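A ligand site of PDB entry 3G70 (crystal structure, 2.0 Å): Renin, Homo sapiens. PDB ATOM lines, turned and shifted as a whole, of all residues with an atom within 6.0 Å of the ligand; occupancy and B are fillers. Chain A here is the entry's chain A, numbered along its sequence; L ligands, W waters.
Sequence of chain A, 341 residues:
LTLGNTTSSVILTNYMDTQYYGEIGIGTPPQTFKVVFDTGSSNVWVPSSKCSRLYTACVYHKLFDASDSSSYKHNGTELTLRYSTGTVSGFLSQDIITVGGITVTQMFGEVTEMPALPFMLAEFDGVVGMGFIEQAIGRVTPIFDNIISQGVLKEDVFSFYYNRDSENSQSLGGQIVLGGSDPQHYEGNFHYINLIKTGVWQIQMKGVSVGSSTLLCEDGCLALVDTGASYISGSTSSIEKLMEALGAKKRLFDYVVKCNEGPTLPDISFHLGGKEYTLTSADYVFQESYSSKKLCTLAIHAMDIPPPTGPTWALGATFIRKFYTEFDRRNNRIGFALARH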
ATOM      1  N   THR A  18      22.107  -3.863 -17.146  1.00  0.00           N
ATOM      2  CA  THR A  18      22.604  -2.888 -16.164  1.00  0.00           C
ATOM      3  C   THR A  18      21.680  -1.705 -15.960  1.00  0.00           C
ATOM      4  O   THR A  18      21.847  -0.961 -14.996  1.00  0.00           O
ATOM      5  CB  THR A  18      24.004  -2.357 -16.539  1.00  0.00           C
ATOM      6  OG1 THR A  18      24.005  -1.934 -17.912  1.00  0.00           O
ATOM      7  CG2 THR A  18      25.051  -3.444 -16.471  1.00  0.00           C
ATOM      8  N   GLN A  19      20.742  -1.519 -16.883  1.00  0.00           N
ATOM      9  CA  GLN A  19      19.823  -0.363 -16.853  1.00  0.00           C
ATOM     10  C   GLN A  19      18.405  -0.771 -17.198  1.00  0.00           C
ATOM     11  O   GLN A  19      18.122  -1.281 -18.280  1.00  0.00           O
ATOM     12  CB  GLN A  19      20.273   0.705 -17.846  1.00  0.00           C
ATOM     13  CG  GLN A  19      21.663   1.270 -17.593  1.00  0.00           C
ATOM     14  CD  GLN A  19      22.084   2.239 -18.679  1.00  0.00           C
ATOM     15  OE1 GLN A  19      21.264   2.976 -19.203  1.00  0.00           O
ATOM     16  NE2 GLN A  19      23.382   2.261 -18.985  1.00  0.00           N
ATOM     17  N   VAL A  36      14.963   5.556 -14.553  1.00  0.00           N
ATOM     18  CA  VAL A  36      15.121   4.481 -13.572  1.00  0.00           C
ATOM     19  C   VAL A  36      14.226   4.765 -12.332  1.00  0.00           C
ATOM     20  O   VAL A  36      14.215   5.850 -11.815  1.00  0.00           O
ATOM     21  CB  VAL A  36      16.634   4.340 -13.090  1.00  0.00           C
ATOM     22  CG1 VAL A  36      16.747   3.357 -11.943  1.00  0.00           C
ATOM     23  CG2 VAL A  36      17.532   3.842 -14.198  1.00  0.00           C
ATOM     24  N   ASP A  38      14.116   4.002  -8.636  1.00  0.00           N
ATOM     25  CA  ASP A  38      15.298   3.778  -7.798  1.00  0.00           C
ATOM     26  C   ASP A  38      14.917   3.758  -6.321  1.00  0.00           C
ATOM     27  O   ASP A  38      14.535   4.772  -5.802  1.00  0.00           O
ATOM     28  CB  ASP A  38      16.256   4.946  -8.021  1.00  0.00           C
ATOM     29  CG  ASP A  38      17.653   4.680  -7.478  1.00  0.00           C
ATOM     30  OD1 ASP A  38      17.813   4.377  -6.310  1.00  0.00           O
ATOM     31  OD2 ASP A  38      18.662   4.745  -8.170  1.00  0.00           O
ATOM     32  N   GLY A  40      17.042   3.376  -3.841  1.00  0.00           N
ATOM     33  CA  GLY A  40      18.143   3.947  -3.069  1.00  0.00           C
ATOM     34  C   GLY A  40      18.243   5.456  -3.053  1.00  0.00           C
ATOM     35  O   GLY A  40      19.257   6.028  -2.616  1.00  0.00           O
ATOM     36  N   SER A  41      17.193   6.127  -3.518  1.00  0.00           N
ATOM     37  CA  SER A  41      17.134   7.548  -3.491  1.00  0.00           C
ATOM     38  C   SER A  41      15.666   7.987  -3.379  1.00  0.00           C
ATOM     39  O   SER A  41      14.761   7.164  -3.602  1.00  0.00           O
ATOM     40  CB  SER A  41      17.854   8.153  -4.712  1.00  0.00           C
ATOM     41  OG  SER A  41      17.166   7.925  -5.928  1.00  0.00           O
ATOM     42  N   TRP A  45      14.564  13.390 -10.565  1.00  0.00           N
ATOM     43  CA  TRP A  45      15.503  14.246 -11.287  1.00  0.00           C
ATOM     44  C   TRP A  45      15.315  14.109 -12.795  1.00  0.00           C
ATOM     45  O   TRP A  45      15.279  12.994 -13.281  1.00  0.00           O
ATOM     46  CB  TRP A  45      16.958  13.822 -11.024  1.00  0.00           C
ATOM     47  CG  TRP A  45      17.535  14.023  -9.640  1.00  0.00           C
ATOM     48  CD1 TRP A  45      17.598  13.090  -8.664  1.00  0.00           C
ATOM     49  CD2 TRP A  45      18.199  15.190  -9.123  1.00  0.00           C
ATOM     50  NE1 TRP A  45      18.243  13.611  -7.559  1.00  0.00           N
ATOM     51  CE2 TRP A  45      18.625  14.894  -7.826  1.00  0.00           C
ATOM     52  CE3 TRP A  45      18.469  16.463  -9.638  1.00  0.00           C
ATOM     53  CZ2 TRP A  45      19.299  15.812  -7.012  1.00  0.00           C
ATOM     54  CZ3 TRP A  45      19.142  17.392  -8.826  1.00  0.00           C
ATOM     55  CH2 TRP A  45      19.553  17.053  -7.529  1.00  0.00           C
ATOM     56  N   VAL A  46      15.186  15.203 -13.536  1.00  0.00           N
ATOM     57  CA  VAL A  46      15.293  15.144 -15.009  1.00  0.00           C
ATOM     58  C   VAL A  46      16.250  16.222 -15.423  1.00  0.00           C
ATOM     59  O   VAL A  46      16.413  17.180 -14.655  1.00  0.00           O
ATOM     60  CB  VAL A  46      13.923  15.319 -15.765  1.00  0.00           C
ATOM     61  CG1 VAL A  46      13.012  14.074 -15.550  1.00  0.00           C
ATOM     62  CG2 VAL A  46      13.231  16.612 -15.338  1.00  0.00           C
ATOM     63  N   PRO A  47      16.870  16.108 -16.614  1.00  0.00           N
ATOM     64  CA  PRO A  47      17.757  17.206 -17.118  1.00  0.00           C
ATOM     65  C   PRO A  47      16.973  18.461 -17.469  1.00  0.00           C
ATOM     66  O   PRO A  47      15.834  18.363 -17.980  1.00  0.00           O
ATOM     67  CB  PRO A  47      18.380  16.622 -18.391  1.00  0.00           C
ATOM     68  CG  PRO A  47      17.967  15.123 -18.459  1.00  0.00           C
ATOM     69  CD  PRO A  47      16.738  15.002 -17.578  1.00  0.00           C
ATOM     70  N   ALA A  57      26.419  14.826 -20.983  1.00  0.00           N
ATOM     71  CA  ALA A  57      25.251  14.196 -20.351  1.00  0.00           C
ATOM     72  C   ALA A  57      23.953  14.920 -20.692  1.00  0.00           C
ATOM     73  O   ALA A  57      22.879  14.337 -20.692  1.00  0.00           O
ATOM     74  CB  ALA A  57      25.431  14.099 -18.840  1.00  0.00           C
ATOM     75  N   CYS A  58      24.029  16.204 -20.997  1.00  0.00           N
ATOM     76  CA  CYS A  58      22.793  16.883 -21.344  1.00  0.00           C
ATOM     77  C   CYS A  58      22.466  16.747 -22.813  1.00  0.00           C
ATOM     78  O   CYS A  58      21.335  16.434 -23.138  1.00  0.00           O
ATOM     79  CB  CYS A  58      22.784  18.336 -20.881  1.00  0.00           C
ATOM     80  SG  CYS A  58      22.528  18.396 -19.098  1.00  0.00           S
ATOM     81  N   HIS A  61      20.507  13.623 -24.047  1.00  0.00           N
ATOM     82  CA  HIS A  61      19.296  13.283 -23.283  1.00  0.00           C
ATOM     83  C   HIS A  61      18.155  14.261 -23.539  1.00  0.00           C
ATOM     84  O   HIS A  61      18.388  15.338 -24.043  1.00  0.00           O
ATOM     85  CB  HIS A  61      19.622  13.159 -21.785  1.00  0.00           C
ATOM     86  CG  HIS A  61      20.490  11.978 -21.468  1.00  0.00           C
ATOM     87  ND1 HIS A  61      21.778  12.096 -21.005  1.00  0.00           N
ATOM     88  CD2 HIS A  61      20.263  10.651 -21.611  1.00  0.00           C
ATOM     89  CE1 HIS A  61      22.298  10.893 -20.853  1.00  0.00           C
ATOM     90  NE2 HIS A  61      21.411   9.998 -21.232  1.00  0.00           N
ATOM     91  N   LEU A  81      23.566  16.991  -5.355  1.00  0.00           N
ATOM     92  CA  LEU A  81      23.961  15.619  -5.023  1.00  0.00           C
ATOM     93  C   LEU A  81      25.478  15.452  -5.257  1.00  0.00           C
ATOM     94  O   LEU A  81      25.983  15.677  -6.345  1.00  0.00           O
ATOM     95  CB  LEU A  81      23.181  14.638  -5.907  1.00  0.00           C
ATOM     96  CG  LEU A  81      22.837  13.196  -5.513  1.00  0.00           C
ATOM     97  CD1 LEU A  81      23.189  12.314  -6.682  1.00  0.00           C
ATOM     98  CD2 LEU A  81      23.515  12.680  -4.235  1.00  0.00           C
ATOM     99  N   TYR A  83      27.854  13.068  -6.094  1.00  0.00           N
ATOM    100  CA  TYR A  83      28.068  11.738  -6.632  1.00  0.00           C
ATOM    101  C   TYR A  83      29.599  11.420  -6.663  1.00  0.00           C
ATOM    102  O   TYR A  83      30.402  12.293  -6.310  1.00  0.00           O
ATOM    103  CB  TYR A  83      27.403  11.659  -8.027  1.00  0.00           C
ATOM    104  CG  TYR A  83      27.446  10.303  -8.682  1.00  0.00           C
ATOM    105  CD1 TYR A  83      28.431  10.001  -9.625  1.00  0.00           C
ATOM    106  CD2 TYR A  83      26.513   9.334  -8.367  1.00  0.00           C
ATOM    107  CE1 TYR A  83      28.491   8.767 -10.225  1.00  0.00           C
ATOM    108  CE2 TYR A  83      26.557   8.068  -8.968  1.00  0.00           C
ATOM    109  CZ  TYR A  83      27.543   7.800  -9.894  1.00  0.00           C
ATOM    110  OH  TYR A  83      27.590   6.566 -10.487  1.00  0.00           O
ATOM    111  N   VAL A  88      26.146  16.675  -9.002  1.00  0.00           N
ATOM    112  CA  VAL A  88      24.974  16.857  -9.854  1.00  0.00           C
ATOM    113  C   VAL A  88      24.176  17.935  -9.151  1.00  0.00           C
ATOM    114  O   VAL A  88      23.833  17.792  -7.976  1.00  0.00           O
ATOM    115  CB  VAL A  88      24.106  15.581 -10.001  1.00  0.00           C
ATOM    116  CG1 VAL A  88      22.888  15.827 -10.939  1.00  0.00           C
ATOM    117  CG2 VAL A  88      24.941  14.377 -10.487  1.00  0.00           C
ATOM    118  N   VAL A 111      18.123  19.179 -13.488  1.00  0.00           N
ATOM    119  CA  VAL A 111      19.592  19.199 -13.526  1.00  0.00           C
ATOM    120  C   VAL A 111      20.215  20.188 -14.559  1.00  0.00           C
ATOM    121  O   VAL A 111      19.950  20.088 -15.768  1.00  0.00           O
ATOM    122  CB  VAL A 111      20.163  17.793 -13.811  1.00  0.00           C
ATOM    123  CG1 VAL A 111      21.670  17.819 -13.837  1.00  0.00           C
ATOM    124  CG2 VAL A 111      19.678  16.757 -12.791  1.00  0.00           C
ATOM    125  N   MET A 114      26.265  18.189 -14.329  1.00  0.00           N
ATOM    126  CA  MET A 114      26.648  16.864 -13.879  1.00  0.00           C
ATOM    127  C   MET A 114      27.863  16.408 -14.666  1.00  0.00           C
ATOM    128  O   MET A 114      28.086  16.881 -15.791  1.00  0.00           O
ATOM    129  CB  MET A 114      25.526  15.842 -14.119  1.00  0.00           C
ATOM    130  CG  MET A 114      24.931  15.842 -15.511  1.00  0.00           C
ATOM    131  SD  MET A 114      23.537  14.683 -15.591  1.00  0.00           S
ATOM    132  CE  MET A 114      22.458  15.609 -16.700  1.00  0.00           C
ATOM    133  N   PRO A 118      29.183   8.773 -14.975  1.00  0.00           N
ATOM    134  CA  PRO A 118      28.734   7.828 -15.988  1.00  0.00           C
ATOM    135  C   PRO A 118      27.563   8.303 -16.851  1.00  0.00           C
ATOM    136  O   PRO A 118      27.117   7.562 -17.738  1.00  0.00           O
ATOM    137  CB  PRO A 118      28.238   6.653 -15.135  1.00  0.00           C
ATOM    138  CG  PRO A 118      27.789   7.294 -13.874  1.00  0.00           C
ATOM    139  CD  PRO A 118      28.590   8.503 -13.646  1.00  0.00           C
ATOM    140  N   PHE A 119      27.077   9.504 -16.568  1.00  0.00           N
ATOM    141  CA  PHE A 119      25.787   9.980 -17.080  1.00  0.00           C
ATOM    142  C   PHE A 119      25.591  10.035 -18.591  1.00  0.00           C
ATOM    143  O   PHE A 119      24.478   9.819 -19.090  1.00  0.00           O
ATOM    144  CB  PHE A 119      25.419  11.287 -16.378  1.00  0.00           C
ATOM    145  CG  PHE A 119      25.364  11.130 -14.895  1.00  0.00           C
ATOM    146  CD1 PHE A 119      24.396  10.312 -14.303  1.00  0.00           C
ATOM    147  CD2 PHE A 119      26.327  11.744 -14.078  1.00  0.00           C
ATOM    148  CE1 PHE A 119      24.353  10.141 -12.921  1.00  0.00           C
ATOM    149  CE2 PHE A 119      26.288  11.562 -12.704  1.00  0.00           C
ATOM    150  CZ  PHE A 119      25.299  10.761 -12.120  1.00  0.00           C
ATOM    151  N   LEU A 121      26.649   7.813 -20.579  1.00  0.00           N
ATOM    152  CA  LEU A 121      26.447   6.396 -20.926  1.00  0.00           C
ATOM    153  C   LEU A 121      25.052   5.839 -20.589  1.00  0.00           C
ATOM    154  O   LEU A 121      24.676   4.752 -21.052  1.00  0.00           O
ATOM    155  CB  LEU A 121      27.502   5.524 -20.244  1.00  0.00           C
ATOM    156  CG  LEU A 121      28.974   5.908 -20.504  1.00  0.00           C
ATOM    157  CD1 LEU A 121      29.890   5.104 -19.612  1.00  0.00           C
ATOM    158  CD2 LEU A 121      29.334   5.714 -21.973  1.00  0.00           C
ATOM    159  N   ALA A 122      24.296   6.590 -19.792  1.00  0.00           N
ATOM    160  CA  ALA A 122      22.920   6.254 -19.421  1.00  0.00           C
ATOM    161  C   ALA A 122      22.021   6.256 -20.649  1.00  0.00           C
ATOM    162  O   ALA A 122      21.973   7.236 -21.393  1.00  0.00           O
ATOM    163  CB  ALA A 122      22.402   7.269 -18.396  1.00  0.00           C
ATOM    164  N   GLU A 123      21.294   5.163 -20.899  1.00  0.00           N
ATOM    165  CA  GLU A 123      20.322   5.143 -22.021  1.00  0.00           C
ATOM    166  C   GLU A 123      19.007   5.870 -21.659  1.00  0.00           C
ATOM    167  O   GLU A 123      18.209   6.221 -22.534  1.00  0.00           O
ATOM    168  CB  GLU A 123      20.019   3.699 -22.472  1.00  0.00           C
ATOM    169  CG  GLU A 123      21.196   2.878 -22.953  1.00  0.00           C
ATOM    170  CD  GLU A 123      21.933   3.515 -24.109  1.00  0.00           C
ATOM    171  OE1 GLU A 123      21.381   3.500 -25.220  1.00  0.00           O
ATOM    172  OE2 GLU A 123      23.059   4.033 -23.904  1.00  0.00           O
ATOM    173  N   PHE A 124      18.811   6.135 -20.377  1.00  0.00           N
ATOM    174  CA  PHE A 124      17.654   6.845 -19.834  1.00  0.00           C
ATOM    175  C   PHE A 124      17.999   8.326 -19.501  1.00  0.00           C
ATOM    176  O   PHE A 124      19.180   8.693 -19.399  1.00  0.00           O
ATOM    177  CB  PHE A 124      17.166   6.099 -18.573  1.00  0.00           C
ATOM    178  CG  PHE A 124      18.236   5.924 -17.534  1.00  0.00           C
ATOM    179  CD1 PHE A 124      19.131   4.860 -17.603  1.00  0.00           C
ATOM    180  CD2 PHE A 124      18.400   6.858 -16.519  1.00  0.00           C
ATOM    181  CE1 PHE A 124      20.151   4.717 -16.658  1.00  0.00           C
ATOM    182  CE2 PHE A 124      19.427   6.736 -15.574  1.00  0.00           C
ATOM    183  CZ  PHE A 124      20.291   5.669 -15.643  1.00  0.00           C
ATOM    184  N   ASP A 125      16.967   9.158 -19.322  1.00  0.00           N
ATOM    185  CA  ASP A 125      17.116  10.584 -19.079  1.00  0.00           C
ATOM    186  C   ASP A 125      17.144  10.960 -17.621  1.00  0.00           C
ATOM    187  O   ASP A 125      17.817  11.892 -17.253  1.00  0.00           O
ATOM    188  CB  ASP A 125      15.947  11.357 -19.723  1.00  0.00           C
ATOM    189  CG  ASP A 125      15.702  10.961 -21.155  1.00  0.00           C
ATOM    190  OD1 ASP A 125      16.592  11.223 -22.005  1.00  0.00           O
ATOM    191  OD2 ASP A 125      14.647  10.365 -21.518  1.00  0.00           O
ATOM    192  N   GLY A 126      16.358  10.269 -16.792  1.00  0.00           N
ATOM    193  CA  GLY A 126      16.235  10.708 -15.422  1.00  0.00           C
ATOM    194  C   GLY A 126      16.063   9.600 -14.418  1.00  0.00           C
ATOM    195  O   GLY A 126      16.284   8.429 -14.718  1.00  0.00           O
ATOM    196  N   VAL A 127      15.650  10.011 -13.225  1.00  0.00           N
ATOM    197  CA  VAL A 127      15.509   9.144 -12.069  1.00  0.00           C
ATOM    198  C   VAL A 127      14.210   9.478 -11.360  1.00  0.00           C
ATOM    199  O   VAL A 127      13.858  10.647 -11.251  1.00  0.00           O
ATOM    200  CB  VAL A 127      16.738   9.317 -11.135  1.00  0.00           C
ATOM    201  CG1 VAL A 127      16.521   8.666  -9.774  1.00  0.00           C
ATOM    202  CG2 VAL A 127      18.024   8.774 -11.803  1.00  0.00           C
ATOM    203  N   LEU A 224      21.168  -2.829   1.541  1.00  0.00           N
ATOM    204  CA  LEU A 224      20.317  -1.883   0.876  1.00  0.00           C
ATOM    205  C   LEU A 224      19.742  -2.580  -0.366  1.00  0.00           C
ATOM    206  O   LEU A 224      20.474  -3.215  -1.110  1.00  0.00           O
ATOM    207  CB  LEU A 224      21.143  -0.641   0.495  1.00  0.00           C
ATOM    208  CG  LEU A 224      20.461   0.503  -0.265  1.00  0.00           C
ATOM    209  CD1 LEU A 224      19.521   1.299   0.625  1.00  0.00           C
ATOM    210  CD2 LEU A 224      21.529   1.428  -0.890  1.00  0.00           C
ATOM    211  N   ASP A 226      18.425  -1.823  -3.693  1.00  0.00           N
ATOM    212  CA  ASP A 226      18.529  -0.640  -4.548  1.00  0.00           C
ATOM    213  C   ASP A 226      18.260  -1.018  -5.980  1.00  0.00           C
ATOM    214  O   ASP A 226      19.135  -1.545  -6.659  1.00  0.00           O
ATOM    215  CB  ASP A 226      19.942  -0.041  -4.418  1.00  0.00           C
ATOM    216  CG  ASP A 226      20.126   1.266  -5.187  1.00  0.00           C
ATOM    217  OD1 ASP A 226      19.176   1.775  -5.856  1.00  0.00           O
ATOM    218  OD2 ASP A 226      21.219   1.896  -5.166  1.00  0.00           O
ATOM    219  N   GLY A 228      18.052   0.782  -8.387  1.00  0.00           N
ATOM    220  CA  GLY A 228      18.773   1.684  -9.250  1.00  0.00           C
ATOM    221  C   GLY A 228      20.246   1.358  -9.363  1.00  0.00           C
ATOM    222  O   GLY A 228      20.968   2.038 -10.084  1.00  0.00           O
ATOM    223  N   ALA A 229      20.683   0.327  -8.623  1.00  0.00           N
ATOM    224  CA  ALA A 229      22.057  -0.183  -8.737  1.00  0.00           C
ATOM    225  C   ALA A 229      22.031  -1.288  -9.771  1.00  0.00           C
ATOM    226  O   ALA A 229      21.100  -2.097  -9.814  1.00  0.00           O
ATOM    227  CB  ALA A 229      22.541  -0.722  -7.403  1.00  0.00           C
ATOM    228  N   SER A 230      23.059  -1.306 -10.617  1.00  0.00           N
ATOM    229  CA  SER A 230      23.247  -2.358 -11.651  1.00  0.00           C
ATOM    230  C   SER A 230      23.647  -3.731 -11.064  1.00  0.00           C
ATOM    231  O   SER A 230      23.206  -4.777 -11.542  1.00  0.00           O
ATOM    232  CB  SER A 230      24.357  -1.907 -12.620  1.00  0.00           C
ATOM    233  OG  SER A 230      24.002  -0.759 -13.379  1.00  0.00           O
ATOM    234  N   MET A 303      31.789  -1.162  -3.729  1.00  0.00           N
ATOM    235  CA  MET A 303      31.364   0.225  -3.532  1.00  0.00           C
ATOM    236  C   MET A 303      31.347   0.561  -2.041  1.00  0.00           C
ATOM    237  O   MET A 303      30.613  -0.058  -1.247  1.00  0.00           O
ATOM    238  CB  MET A 303      29.992   0.482  -4.151  1.00  0.00           C
ATOM    239  CG  MET A 303      29.728   1.965  -4.378  1.00  0.00           C
ATOM    240  SD  MET A 303      28.537   2.361  -5.684  1.00  0.00           S
ATOM    241  CE  MET A 303      27.118   2.894  -4.719  1.00  0.00           C
HETATM  242 CL1  LIG L   1      24.622   4.624 -16.692  1.00  0.00          CL
HETATM  243  C1  LIG L   1      24.140   4.269 -14.998  1.00  0.00           C
HETATM  244  C2  LIG L   1      23.900   5.329 -14.141  1.00  0.00           C
HETATM  245 CL2  LIG L   1      24.090   7.009 -14.740  1.00  0.00          CL
HETATM  246  C3  LIG L   1      23.981   2.957 -14.548  1.00  0.00           C
HETATM  247  C4  LIG L   1      23.610   2.710 -13.233  1.00  0.00           C
HETATM  248  C5  LIG L   1      23.388   3.783 -12.372  1.00  0.00           C
HETATM  249  C6  LIG L   1      23.525   5.093 -12.818  1.00  0.00           C
HETATM  250  C7  LIG L   1      23.290   6.289 -11.943  1.00  0.00           C
HETATM  251  N1  LIG L   1      22.451   6.124 -10.760  1.00  0.00           N
HETATM  252  C8  LIG L   1      21.041   6.470 -11.030  1.00  0.00           C
HETATM  253  C9  LIG L   1      20.438   5.479 -12.035  1.00  0.00           C
HETATM  254  C10 LIG L   1      20.125   5.355 -10.556  1.00  0.00           C
HETATM  255  C11 LIG L   1      23.000   5.784  -9.565  1.00  0.00           C
HETATM  256  O1  LIG L   1      24.229   5.542  -9.483  1.00  0.00           O
HETATM  257  C12 LIG L   1      22.222   5.678  -8.305  1.00  0.00           C
HETATM  258  C13 LIG L   1      22.195   4.335  -7.617  1.00  0.00           C
HETATM  259  N2  LIG L   1      21.014   4.183  -6.770  1.00  0.00           N
HETATM  260  C14 LIG L   1      20.981   5.210  -5.746  1.00  0.00           C
HETATM  261  C15 LIG L   1      20.823   6.589  -6.403  1.00  0.00           C
HETATM  262  C16 LIG L   1      23.457   4.140  -6.777  1.00  0.00           C
HETATM  263  N3  LIG L   1      23.479   5.139  -5.711  1.00  0.00           N
HETATM  264  C17 LIG L   1      22.265   5.112  -4.889  1.00  0.00           C
HETATM  265  C18 LIG L   1      21.582   6.744  -7.728  1.00  0.00           C
HETATM  266  C19 LIG L   1      21.543   8.157  -8.308  1.00  0.00           C
HETATM  267  C20 LIG L   1      22.654   8.770  -8.882  1.00  0.00           C
HETATM  268  C21 LIG L   1      22.559  10.065  -9.392  1.00  0.00           C
HETATM  269  C22 LIG L   1      20.350   8.874  -8.233  1.00  0.00           C
HETATM  270  C23 LIG L   1      20.246  10.173  -8.715  1.00  0.00           C
HETATM  271  C24 LIG L   1      21.361  10.775  -9.297  1.00  0.00           C
HETATM  272  C25 LIG L   1      21.263  12.147  -9.838  1.00  0.00           C
HETATM  273  C26 LIG L   1      21.217  12.368 -11.161  1.00  0.00           C
HETATM  274  C27 LIG L   1      20.737  11.326 -12.129  1.00  0.00           C
HETATM  275  O2  LIG L   1      19.873  11.851 -13.152  1.00  0.00           O
HETATM  276  C28 LIG L   1      20.290  11.391 -14.402  1.00  0.00           C
HETATM  277  C29 LIG L   1      20.733  10.086 -14.666  1.00  0.00           C
HETATM  278  F1  LIG L   1      20.806   9.173 -13.699  1.00  0.00           F
HETATM  279  C30 LIG L   1      20.256  12.276 -15.448  1.00  0.00           C
HETATM  280 CL3  LIG L   1      19.658  13.928 -15.063  1.00  0.00          CL
HETATM  281  C31 LIG L   1      20.662  11.881 -16.730  1.00  0.00           C
HETATM  282  F2  LIG L   1      20.628  12.738 -17.762  1.00  0.00           F
HETATM  283  C32 LIG L   1      21.100  10.598 -16.987  1.00  0.00           C
HETATM  284  C33 LIG L   1      21.154   9.705 -15.934  1.00  0.00           C
HETATM  285  O   HOH W   1      25.926   0.350 -14.877  1.00  0.00           O
HETATM  286  O   HOH W   2      24.702   3.428  -2.970  1.00  0.00           O
HETATM  287  O   HOH W   3      23.807   8.343  -5.605  1.00  0.00           O
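A fluorine (F2) of the ligand sits close to the backbone carbonyl oxygen of Asp 125 (3.0 Å).
Residues that only touch the ligand: Phe 119 (3.3 Å), Phe 124 (3.4 Å), Val 127 (3.4 Å), Gly 228 (3.5 Å), Tyr 83 (3.5 Å), Ser 230 (3.5 Å), His 61 (3.5 Å), Gln 19 (3.5 Å), Leu 81 (3.5 Å), Met 114 (3.6 Å), Ala 122 (3.6 Å), Val 111 (3.6 Å), Pro 47 (3.6 Å), Gly 40 (3.7 Å), Ser 41 (3.8 Å), Pro 118 (3.8 Å), Val 88 (3.8 Å), Trp 45 (3.9 Å) and Val 36 (3.98 Å).
Hydrophobic or aromatic side chains that line the ligand: Val 36, Trp 45, Pro 47, His 61, Leu 81, Tyr 83, Val 88, Val 111, Met 114, Pro 118, Phe 119, Ala 122, Phe 124 and Val 127.
Within 4 Å of the ligand: Gln 19, Val 36, Asp 38, Gly 40, Ser 41, Trp 45, Pro 47, His 61, Leu 81, Tyr 83, Val 88, Val 111, Met 114, Pro 118, Phe 119, Ala 122, Phe 124, Asp 125, Val 127, Asp 226, Gly 228 and Ser 230.
The nearest printed residue that does not touch the ligand is Ala 57 (4.03 Å).
The side-chain carboxylate (OD2) of Asp 38 lies within salt-bridge range of a nitrogen (N2) of the ligand (2.8 Å).
OD2 of Asp 226 is in salt-bridge range of N2 of the ligand (2.8 Å).
The side-chain carboxylate (OD1) of Asp 38 is in hydrogen-bond range of the backbone NH (N) of Ser 41, at 3.4 Å.
The backbone NH (N) of Ala 229 lies within hydrogen-bond range of the side-chain carboxylate (OD1) of Asp 226 (3.5 Å).
NE2 of His 61 sits close to O of Phe 124, at 3.2 Å.
O of Val 127 lies within hydrogen-bond range of N of Trp 45 (2.9 Å).
A ring nitrogen (ND1) of His 61 is in hydrogen-bond range of the backbone carbonyl oxygen (O) of Ala 57 (2.5 Å).
O of Leu 121 lies within hydrogen-bond range of NE2 of Gln 19 (3.5 Å).
N of Val 111 sits at hydrogen-bond distance from O of Val 46.
The backbone NH (N) of Val 36 is in hydrogen-bond range of the backbone carbonyl oxygen (O) of Gly 126 (3.2 Å).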
